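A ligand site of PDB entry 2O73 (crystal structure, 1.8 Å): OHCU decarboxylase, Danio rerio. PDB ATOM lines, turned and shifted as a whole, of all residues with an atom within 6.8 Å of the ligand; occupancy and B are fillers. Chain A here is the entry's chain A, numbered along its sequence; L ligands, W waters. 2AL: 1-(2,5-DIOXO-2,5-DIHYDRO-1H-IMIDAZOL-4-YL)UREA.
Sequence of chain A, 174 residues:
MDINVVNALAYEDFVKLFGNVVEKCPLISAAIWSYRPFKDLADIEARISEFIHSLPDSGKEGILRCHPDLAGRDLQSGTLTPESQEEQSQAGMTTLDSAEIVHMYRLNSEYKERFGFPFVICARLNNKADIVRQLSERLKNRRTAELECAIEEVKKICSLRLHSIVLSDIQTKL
NE2 of Gln 88 sits at hydrogen-bond distance from O5 of the ligand, at 3.2 Å.
OE1 of Glu 87 sits at hydrogen-bond distance from N7 of the ligand, 2.7 Å away.
The side-chain hydroxyl (OG) of Ser 84 lies within hydrogen-bond range of an oxygen (O5) of the ligand (3.2 Å).
O of Ile 121 is in hydrogen-bond range of N1 of the ligand (3.3 Å).
An oxygen (O8) of the ligand lies within hydrogen-bond range of the backbone NH (N) of Ala 123, 3.0 Å away.
O of Pro 68 sits at hydrogen-bond distance from N3 of the ligand, 3.5 Å away.
The side-chain amide nitrogen (NE2) of Gln 88 lies within hydrogen-bond range of the backbone carbonyl oxygen (O) of Asp 69 (3.1 Å).
The guanidinium group of Arg 161 is in salt-bridge range of the side-chain carboxylate of Glu 87, at 2.8 Å.
The side-chain amide nitrogen of Asn 108 lies within hydrogen-bond range of the backbone carbonyl oxygen of Leu 70 (3.2 Å).
OE2 of Glu 23 sits at hydrogen-bond distance from OG of Ser 84 (2.8 Å).
OG of Ser 84 lies within hydrogen-bond range of NH2 of Arg 161.
The backbone NH (N) of Cys 122 lies within hydrogen-bond range of the side-chain carboxylate (OE1) of Glu 153 (2.9 Å).
The backbone NH of Ser 84 sits at hydrogen-bond distance from the side-chain hydroxyl of Thr 81, at 3.3 Å.
O2 of the ligand lies close to O of Phe 119, 3.0 Å away.
Merely in contact with the ligand: Leu 70 (3.5 Å), Val 120 (3.5 Å), Cys 122 (3.9 Å) and Ile 157 (3.3 Å).
Hydrophobic or aromatic side chains that line the ligand: Leu 70, Val 120, Ala 123 and Ile 157.
11 residues have an atom within 4 Å of the ligand: Pro 68, Leu 70, Ser 84, Glu 87, Gln 88, Phe 119, Val 120, Ile 121, Cys 122, Ala 123 and Ile 157.
Water W1 lies within hydrogen-bond range of an oxygen (O8) of the ligand (2.9 Å), the backbone NH (N) of Arg 124 (2.9 Å), the backbone NH (N) of Ala 123 (3.2 Å) and the side-chain sulfur (SG) of Cys 122 (3.4 Å).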
ATOM      1  N   GLU A  23      -0.757 -19.802 -27.847  1.00  0.00           N
ATOM      2  CA  GLU A  23      -1.982 -20.606 -27.709  1.00  0.00           C
ATOM      3  C   GLU A  23      -2.911 -20.610 -28.934  1.00  0.00           C
ATOM      4  O   GLU A  23      -3.417 -19.558 -29.339  1.00  0.00           O
ATOM      5  CB  GLU A  23      -2.770 -20.159 -26.477  1.00  0.00           C
ATOM      6  CG  GLU A  23      -4.055 -20.983 -26.227  1.00  0.00           C
ATOM      7  CD  GLU A  23      -3.799 -22.337 -25.568  1.00  0.00           C
ATOM      8  OE1 GLU A  23      -2.648 -22.838 -25.574  1.00  0.00           O
ATOM      9  OE2 GLU A  23      -4.782 -22.923 -25.039  1.00  0.00           O
ATOM     10  N   LEU A  64      -5.133 -12.909 -28.603  1.00  0.00           N
ATOM     11  CA  LEU A  64      -5.681 -12.910 -27.249  1.00  0.00           C
ATOM     12  C   LEU A  64      -7.003 -13.715 -27.178  1.00  0.00           C
ATOM     13  O   LEU A  64      -7.234 -14.495 -26.239  1.00  0.00           O
ATOM     14  CB  LEU A  64      -5.880 -11.465 -26.791  1.00  0.00           C
ATOM     15  CG  LEU A  64      -4.612 -10.606 -26.682  1.00  0.00           C
ATOM     16  CD1 LEU A  64      -4.933  -9.154 -26.350  1.00  0.00           C
ATOM     17  CD2 LEU A  64      -3.617 -11.194 -25.677  1.00  0.00           C
ATOM     18  N   HIS A  67      -6.995 -17.426 -26.581  1.00  0.00           N
ATOM     19  CA  HIS A  67      -6.619 -17.937 -25.251  1.00  0.00           C
ATOM     20  C   HIS A  67      -7.860 -18.280 -24.429  1.00  0.00           C
ATOM     21  O   HIS A  67      -8.876 -17.579 -24.486  1.00  0.00           O
ATOM     22  CB  HIS A  67      -5.771 -16.923 -24.500  1.00  0.00           C
ATOM     23  CG  HIS A  67      -4.366 -16.799 -24.998  1.00  0.00           C
ATOM     24  ND1 HIS A  67      -4.038 -16.118 -26.160  1.00  0.00           N
ATOM     25  CD2 HIS A  67      -3.192 -17.257 -24.493  1.00  0.00           C
ATOM     26  CE1 HIS A  67      -2.730 -16.174 -26.342  1.00  0.00           C
ATOM     27  NE2 HIS A  67      -2.187 -16.846 -25.345  1.00  0.00           N
ATOM     28  N   PRO A  68      -7.791 -19.367 -23.648  1.00  0.00           N
ATOM     29  CA  PRO A  68      -8.933 -19.660 -22.789  1.00  0.00           C
ATOM     30  C   PRO A  68      -8.914 -18.806 -21.543  1.00  0.00           C
ATOM     31  O   PRO A  68      -7.881 -18.281 -21.167  1.00  0.00           O
ATOM     32  CB  PRO A  68      -8.723 -21.134 -22.422  1.00  0.00           C
ATOM     33  CG  PRO A  68      -7.230 -21.340 -22.482  1.00  0.00           C
ATOM     34  CD  PRO A  68      -6.722 -20.382 -23.535  1.00  0.00           C
ATOM     35  N   ASP A  69     -10.082 -18.653 -20.905  1.00  0.00           N
ATOM     36  CA  ASP A  69     -10.138 -17.941 -19.635  1.00  0.00           C
ATOM     37  C   ASP A  69      -9.476 -18.761 -18.526  1.00  0.00           C
ATOM     38  O   ASP A  69      -9.566 -20.007 -18.495  1.00  0.00           O
ATOM     39  CB  ASP A  69     -11.584 -17.685 -19.229  1.00  0.00           C
ATOM     40  CG  ASP A  69     -12.170 -16.431 -19.860  1.00  0.00           C
ATOM     41  OD1 ASP A  69     -11.513 -15.784 -20.719  1.00  0.00           O
ATOM     42  OD2 ASP A  69     -13.320 -16.097 -19.504  1.00  0.00           O
ATOM     43  N   LEU A  70      -8.784 -18.068 -17.635  1.00  0.00           N
ATOM     44  CA  LEU A  70      -8.342 -18.663 -16.379  1.00  0.00           C
ATOM     45  C   LEU A  70      -9.563 -19.186 -15.600  1.00  0.00           C
ATOM     46  O   LEU A  70     -10.502 -18.441 -15.347  1.00  0.00           O
ATOM     47  CB  LEU A  70      -7.613 -17.606 -15.558  1.00  0.00           C
ATOM     48  CG  LEU A  70      -6.251 -17.160 -16.102  1.00  0.00           C
ATOM     49  CD1 LEU A  70      -5.833 -15.848 -15.469  1.00  0.00           C
ATOM     50  CD2 LEU A  70      -5.212 -18.227 -15.847  1.00  0.00           C
ATOM     51  N   LEU A  80      -8.831 -27.990 -22.116  1.00  0.00           N
ATOM     52  CA  LEU A  80      -7.659 -27.144 -22.367  1.00  0.00           C
ATOM     53  C   LEU A  80      -6.602 -27.909 -23.124  1.00  0.00           C
ATOM     54  O   LEU A  80      -6.534 -29.145 -23.062  1.00  0.00           O
ATOM     55  CB  LEU A  80      -7.052 -26.612 -21.060  1.00  0.00           C
ATOM     56  CG  LEU A  80      -7.895 -25.610 -20.303  1.00  0.00           C
ATOM     57  CD1 LEU A  80      -9.251 -26.232 -20.206  1.00  0.00           C
ATOM     58  CD2 LEU A  80      -7.356 -25.298 -18.936  1.00  0.00           C
ATOM     59  N   THR A  81      -5.763 -27.164 -23.840  1.00  0.00           N
ATOM     60  CA  THR A  81      -4.532 -27.707 -24.409  1.00  0.00           C
ATOM     61  C   THR A  81      -3.673 -28.193 -23.242  1.00  0.00           C
ATOM     62  O   THR A  81      -3.811 -27.705 -22.106  1.00  0.00           O
ATOM     63  CB  THR A  81      -3.776 -26.638 -25.209  1.00  0.00           C
ATOM     64  OG1 THR A  81      -3.416 -25.550 -24.342  1.00  0.00           O
ATOM     65  CG2 THR A  81      -4.641 -26.093 -26.364  1.00  0.00           C
ATOM     66  N   GLU A  83      -0.586 -27.577 -22.410  1.00  0.00           N
ATOM     67  CA  GLU A  83       0.165 -26.468 -21.805  1.00  0.00           C
ATOM     68  C   GLU A  83      -0.725 -25.583 -20.945  1.00  0.00           C
ATOM     69  O   GLU A  83      -0.417 -25.317 -19.792  1.00  0.00           O
ATOM     70  CB  GLU A  83       0.856 -25.600 -22.879  1.00  0.00           C
ATOM     71  CG  GLU A  83       1.861 -26.315 -23.790  1.00  0.00           C
ATOM     72  CD  GLU A  83       1.227 -26.944 -25.036  1.00  0.00           C
ATOM     73  OE1 GLU A  83       0.055 -27.411 -24.973  1.00  0.00           O
ATOM     74  OE2 GLU A  83       1.906 -26.997 -26.078  1.00  0.00           O
ATOM     75  N   SER A  84      -1.840 -25.103 -21.516  1.00  0.00           N
ATOM     76  CA  SER A  84      -2.781 -24.312 -20.726  1.00  0.00           C
ATOM     77  C   SER A  84      -3.219 -25.066 -19.447  1.00  0.00           C
ATOM     78  O   SER A  84      -3.284 -24.477 -18.384  1.00  0.00           O
ATOM     79  CB  SER A  84      -4.005 -23.925 -21.564  1.00  0.00           C
ATOM     80  OG  SER A  84      -3.718 -22.806 -22.408  1.00  0.00           O
ATOM     81  N   GLN A  85      -3.497 -26.363 -19.577  1.00  0.00           N
ATOM     82  CA  GLN A  85      -3.926 -27.163 -18.437  1.00  0.00           C
ATOM     83  C   GLN A  85      -2.873 -27.173 -17.332  1.00  0.00           C
ATOM     84  O   GLN A  85      -3.174 -26.882 -16.168  1.00  0.00           O
ATOM     85  CB  GLN A  85      -4.280 -28.602 -18.867  1.00  0.00           C
ATOM     86  CG  GLN A  85      -4.585 -29.550 -17.709  1.00  0.00           C
ATOM     87  CD  GLN A  85      -5.834 -29.162 -16.923  1.00  0.00           C
ATOM     88  OE1 GLN A  85      -6.882 -28.854 -17.504  1.00  0.00           O
ATOM     89  NE2 GLN A  85      -5.717 -29.169 -15.597  1.00  0.00           N
ATOM     90  N   GLU A  87      -0.436 -25.099 -16.971  1.00  0.00           N
ATOM     91  CA  GLU A  87      -0.141 -23.715 -16.587  1.00  0.00           C
ATOM     92  C   GLU A  87      -1.148 -23.156 -15.597  1.00  0.00           C
ATOM     93  O   GLU A  87      -0.783 -22.415 -14.680  1.00  0.00           O
ATOM     94  CB  GLU A  87      -0.074 -22.807 -17.831  1.00  0.00           C
ATOM     95  CG  GLU A  87       1.238 -22.911 -18.621  1.00  0.00           C
ATOM     96  CD  GLU A  87       1.112 -22.451 -20.084  1.00  0.00           C
ATOM     97  OE1 GLU A  87       0.064 -21.852 -20.464  1.00  0.00           O
ATOM     98  OE2 GLU A  87       2.060 -22.685 -20.851  1.00  0.00           O
ATOM     99  N   GLN A  88      -2.422 -23.494 -15.797  1.00  0.00           N
ATOM    100  CA  GLN A  88      -3.487 -23.122 -14.870  1.00  0.00           C
ATOM    101  C   GLN A  88      -3.418 -23.937 -13.578  1.00  0.00           C
ATOM    102  O   GLN A  88      -3.726 -23.413 -12.505  1.00  0.00           O
ATOM    103  CB  GLN A  88      -4.878 -23.245 -15.522  1.00  0.00           C
ATOM    104  CG  GLN A  88      -5.067 -22.357 -16.763  1.00  0.00           C
ATOM    105  CD  GLN A  88      -6.501 -21.860 -16.952  1.00  0.00           C
ATOM    106  OE1 GLN A  88      -7.268 -21.743 -15.987  1.00  0.00           O
ATOM    107  NE2 GLN A  88      -6.868 -21.538 -18.205  1.00  0.00           N
ATOM    108  N   ASN A 108     -13.546 -12.204 -14.966  1.00  0.00           N
ATOM    109  CA  ASN A 108     -13.325 -12.390 -16.385  1.00  0.00           C
ATOM    110  C   ASN A 108     -14.406 -11.753 -17.242  1.00  0.00           C
ATOM    111  O   ASN A 108     -14.118 -11.133 -18.273  1.00  0.00           O
ATOM    112  CB  ASN A 108     -13.145 -13.854 -16.694  1.00  0.00           C
ATOM    113  CG  ASN A 108     -11.715 -14.285 -16.534  1.00  0.00           C
ATOM    114  OD1 ASN A 108     -10.803 -13.569 -16.945  1.00  0.00           O
ATOM    115  ND2 ASN A 108     -11.511 -15.441 -15.935  1.00  0.00           N
ATOM    116  N   PRO A 118     -10.009 -11.767 -23.965  1.00  0.00           N
ATOM    117  CA  PRO A 118      -9.825 -12.337 -22.624  1.00  0.00           C
ATOM    118  C   PRO A 118      -8.723 -11.658 -21.861  1.00  0.00           C
ATOM    119  O   PRO A 118      -7.810 -11.046 -22.440  1.00  0.00           O
ATOM    120  CB  PRO A 118      -9.449 -13.791 -22.902  1.00  0.00           C
ATOM    121  CG  PRO A 118      -9.817 -14.041 -24.372  1.00  0.00           C
ATOM    122  CD  PRO A 118      -9.639 -12.704 -25.029  1.00  0.00           C
ATOM    123  N   PHE A 119      -8.832 -11.729 -20.532  1.00  0.00           N
ATOM    124  CA  PHE A 119      -7.718 -11.417 -19.658  1.00  0.00           C
ATOM    125  C   PHE A 119      -6.635 -12.471 -19.817  1.00  0.00           C
ATOM    126  O   PHE A 119      -6.875 -13.669 -19.657  1.00  0.00           O
ATOM    127  CB  PHE A 119      -8.179 -11.423 -18.201  1.00  0.00           C
ATOM    128  CG  PHE A 119      -7.045 -11.272 -17.226  1.00  0.00           C
ATOM    129  CD1 PHE A 119      -6.486 -10.025 -16.979  1.00  0.00           C
ATOM    130  CD2 PHE A 119      -6.530 -12.375 -16.549  1.00  0.00           C
ATOM    131  CE1 PHE A 119      -5.428  -9.874 -16.064  1.00  0.00           C
ATOM    132  CE2 PHE A 119      -5.483 -12.233 -15.645  1.00  0.00           C
ATOM    133  CZ  PHE A 119      -4.932 -10.982 -15.402  1.00  0.00           C
ATOM    134  N   VAL A 120      -5.430 -12.024 -20.171  1.00  0.00           N
ATOM    135  CA  VAL A 120      -4.335 -12.963 -20.370  1.00  0.00           C
ATOM    136  C   VAL A 120      -3.176 -12.607 -19.435  1.00  0.00           C
ATOM    137  O   VAL A 120      -2.728 -11.469 -19.399  1.00  0.00           O
ATOM    138  CB  VAL A 120      -3.842 -13.025 -21.849  1.00  0.00           C
ATOM    139  CG1 VAL A 120      -2.592 -13.902 -21.951  1.00  0.00           C
ATOM    140  CG2 VAL A 120      -4.964 -13.570 -22.757  1.00  0.00           C
ATOM    141  N   ILE A 121      -2.710 -13.589 -18.689  1.00  0.00           N
ATOM    142  CA  ILE A 121      -1.533 -13.389 -17.838  1.00  0.00           C
ATOM    143  C   ILE A 121      -0.621 -14.600 -17.946  1.00  0.00           C
ATOM    144  O   ILE A 121      -1.086 -15.717 -18.216  1.00  0.00           O
ATOM    145  CB  ILE A 121      -1.938 -13.138 -16.370  1.00  0.00           C
ATOM    146  CG1 ILE A 121      -0.773 -12.549 -15.570  1.00  0.00           C
ATOM    147  CG2 ILE A 121      -2.429 -14.428 -15.730  1.00  0.00           C
ATOM    148  CD1 ILE A 121      -1.180 -12.034 -14.199  1.00  0.00           C
ATOM    149  N   CYS A 122       0.677 -14.401 -17.741  1.00  0.00           N
ATOM    150  CA  CYS A 122       1.580 -15.548 -17.697  1.00  0.00           C
ATOM    151  C   CYS A 122       1.309 -16.373 -16.420  1.00  0.00           C
ATOM    152  O   CYS A 122       1.768 -16.017 -15.333  1.00  0.00           O
ATOM    153  CB  CYS A 122       3.046 -15.086 -17.762  1.00  0.00           C
ATOM    154  SG  CYS A 122       4.215 -16.426 -17.967  1.00  0.00           S
ATOM    155  N   ALA A 123       0.565 -17.468 -16.551  1.00  0.00           N
ATOM    156  CA  ALA A 123       0.108 -18.237 -15.378  1.00  0.00           C
ATOM    157  C   ALA A 123       1.231 -18.930 -14.595  1.00  0.00           C
ATOM    158  O   ALA A 123       1.125 -19.148 -13.383  1.00  0.00           O
ATOM    159  CB  ALA A 123      -0.968 -19.256 -15.776  1.00  0.00           C
ATOM    160  N   ARG A 124       2.310 -19.294 -15.281  1.00  0.00           N
ATOM    161  CA  ARG A 124       3.423 -19.980 -14.626  1.00  0.00           C
ATOM    162  C   ARG A 124       4.277 -19.048 -13.753  1.00  0.00           C
ATOM    163  O   ARG A 124       5.167 -19.519 -13.017  1.00  0.00           O
ATOM    164  CB  ARG A 124       4.283 -20.716 -15.642  1.00  0.00           C
ATOM    165  CG  ARG A 124       3.721 -22.083 -15.976  1.00  0.00           C
ATOM    166  CD  ARG A 124       4.862 -23.080 -16.150  1.00  0.00           C
ATOM    167  NE  ARG A 124       5.309 -23.173 -17.529  1.00  0.00           N
ATOM    168  CZ  ARG A 124       6.532 -23.537 -17.906  1.00  0.00           C
ATOM    169  NH1 ARG A 124       7.462 -23.807 -17.000  1.00  0.00           N
ATOM    170  NH2 ARG A 124       6.833 -23.610 -19.186  1.00  0.00           N
ATOM    171  N   GLU A 153       2.361 -10.300 -22.193  1.00  0.00           N
ATOM    172  CA  GLU A 153       2.111 -11.500 -21.434  1.00  0.00           C
ATOM    173  C   GLU A 153       2.107 -12.691 -22.358  1.00  0.00           C
ATOM    174  O   GLU A 153       2.599 -13.746 -22.017  1.00  0.00           O
ATOM    175  CB  GLU A 153       0.774 -11.421 -20.686  1.00  0.00           C
ATOM    176  CG  GLU A 153       0.763 -10.421 -19.535  1.00  0.00           C
ATOM    177  CD  GLU A 153       1.866 -10.692 -18.502  1.00  0.00           C
ATOM    178  OE1 GLU A 153       1.917 -11.801 -17.943  1.00  0.00           O
ATOM    179  OE2 GLU A 153       2.663  -9.773 -18.252  1.00  0.00           O
ATOM    180  N   ILE A 157       4.452 -16.061 -21.939  1.00  0.00           N
ATOM    181  CA  ILE A 157       3.962 -17.434 -21.970  1.00  0.00           C
ATOM    182  C   ILE A 157       4.723 -18.245 -23.022  1.00  0.00           C
ATOM    183  O   ILE A 157       5.154 -19.378 -22.762  1.00  0.00           O
ATOM    184  CB  ILE A 157       2.428 -17.454 -22.271  1.00  0.00           C
ATOM    185  CG1 ILE A 157       1.661 -16.739 -21.153  1.00  0.00           C
ATOM    186  CG2 ILE A 157       1.947 -18.866 -22.457  1.00  0.00           C
ATOM    187  CD1 ILE A 157       0.175 -16.516 -21.460  1.00  0.00           C
ATOM    188  N   ARG A 161       6.921 -21.646 -22.606  1.00  0.00           N
ATOM    189  CA  ARG A 161       6.584 -22.820 -23.428  1.00  0.00           C
ATOM    190  C   ARG A 161       7.778 -23.305 -24.235  1.00  0.00           C
ATOM    191  O   ARG A 161       8.033 -24.508 -24.325  1.00  0.00           O
ATOM    192  CB  ARG A 161       5.392 -22.516 -24.364  1.00  0.00           C
ATOM    193  CG  ARG A 161       4.074 -22.407 -23.603  1.00  0.00           C
ATOM    194  CD  ARG A 161       2.838 -22.370 -24.492  1.00  0.00           C
ATOM    195  NE  ARG A 161       1.653 -22.311 -23.637  1.00  0.00           N
ATOM    196  CZ  ARG A 161       0.392 -22.294 -24.065  1.00  0.00           C
ATOM    197  NH1 ARG A 161       0.123 -22.340 -25.359  1.00  0.00           N
ATOM    198  NH2 ARG A 161      -0.592 -22.224 -23.165  1.00  0.00           N
HETATM  199  C4  2AL L   1      -3.643 -18.802 -19.030  1.00  0.00           C
HETATM  200  C5  2AL L   1      -3.235 -20.216 -19.442  1.00  0.00           C
HETATM  201  O5  2AL L   1      -4.007 -21.152 -19.662  1.00  0.00           O
HETATM  202  N7  2AL L   1      -1.911 -20.285 -19.467  1.00  0.00           N
HETATM  203  C8  2AL L   1      -1.420 -19.081 -19.156  1.00  0.00           C
HETATM  204  O8  2AL L   1      -0.211 -18.839 -19.088  1.00  0.00           O
HETATM  205  N9  2AL L   1      -2.337 -18.151 -18.908  1.00  0.00           N
HETATM  206  N3  2AL L   1      -4.644 -18.149 -19.907  1.00  0.00           N
HETATM  207  C2  2AL L   1      -4.969 -16.868 -19.764  1.00  0.00           C
HETATM  208  N1  2AL L   1      -4.295 -16.169 -18.859  1.00  0.00           N
HETATM  209  O2  2AL L   1      -5.842 -16.326 -20.452  1.00  0.00           O
HETATM  210  O   HOH W   1       2.513 -19.372 -18.210  1.00  0.00           O
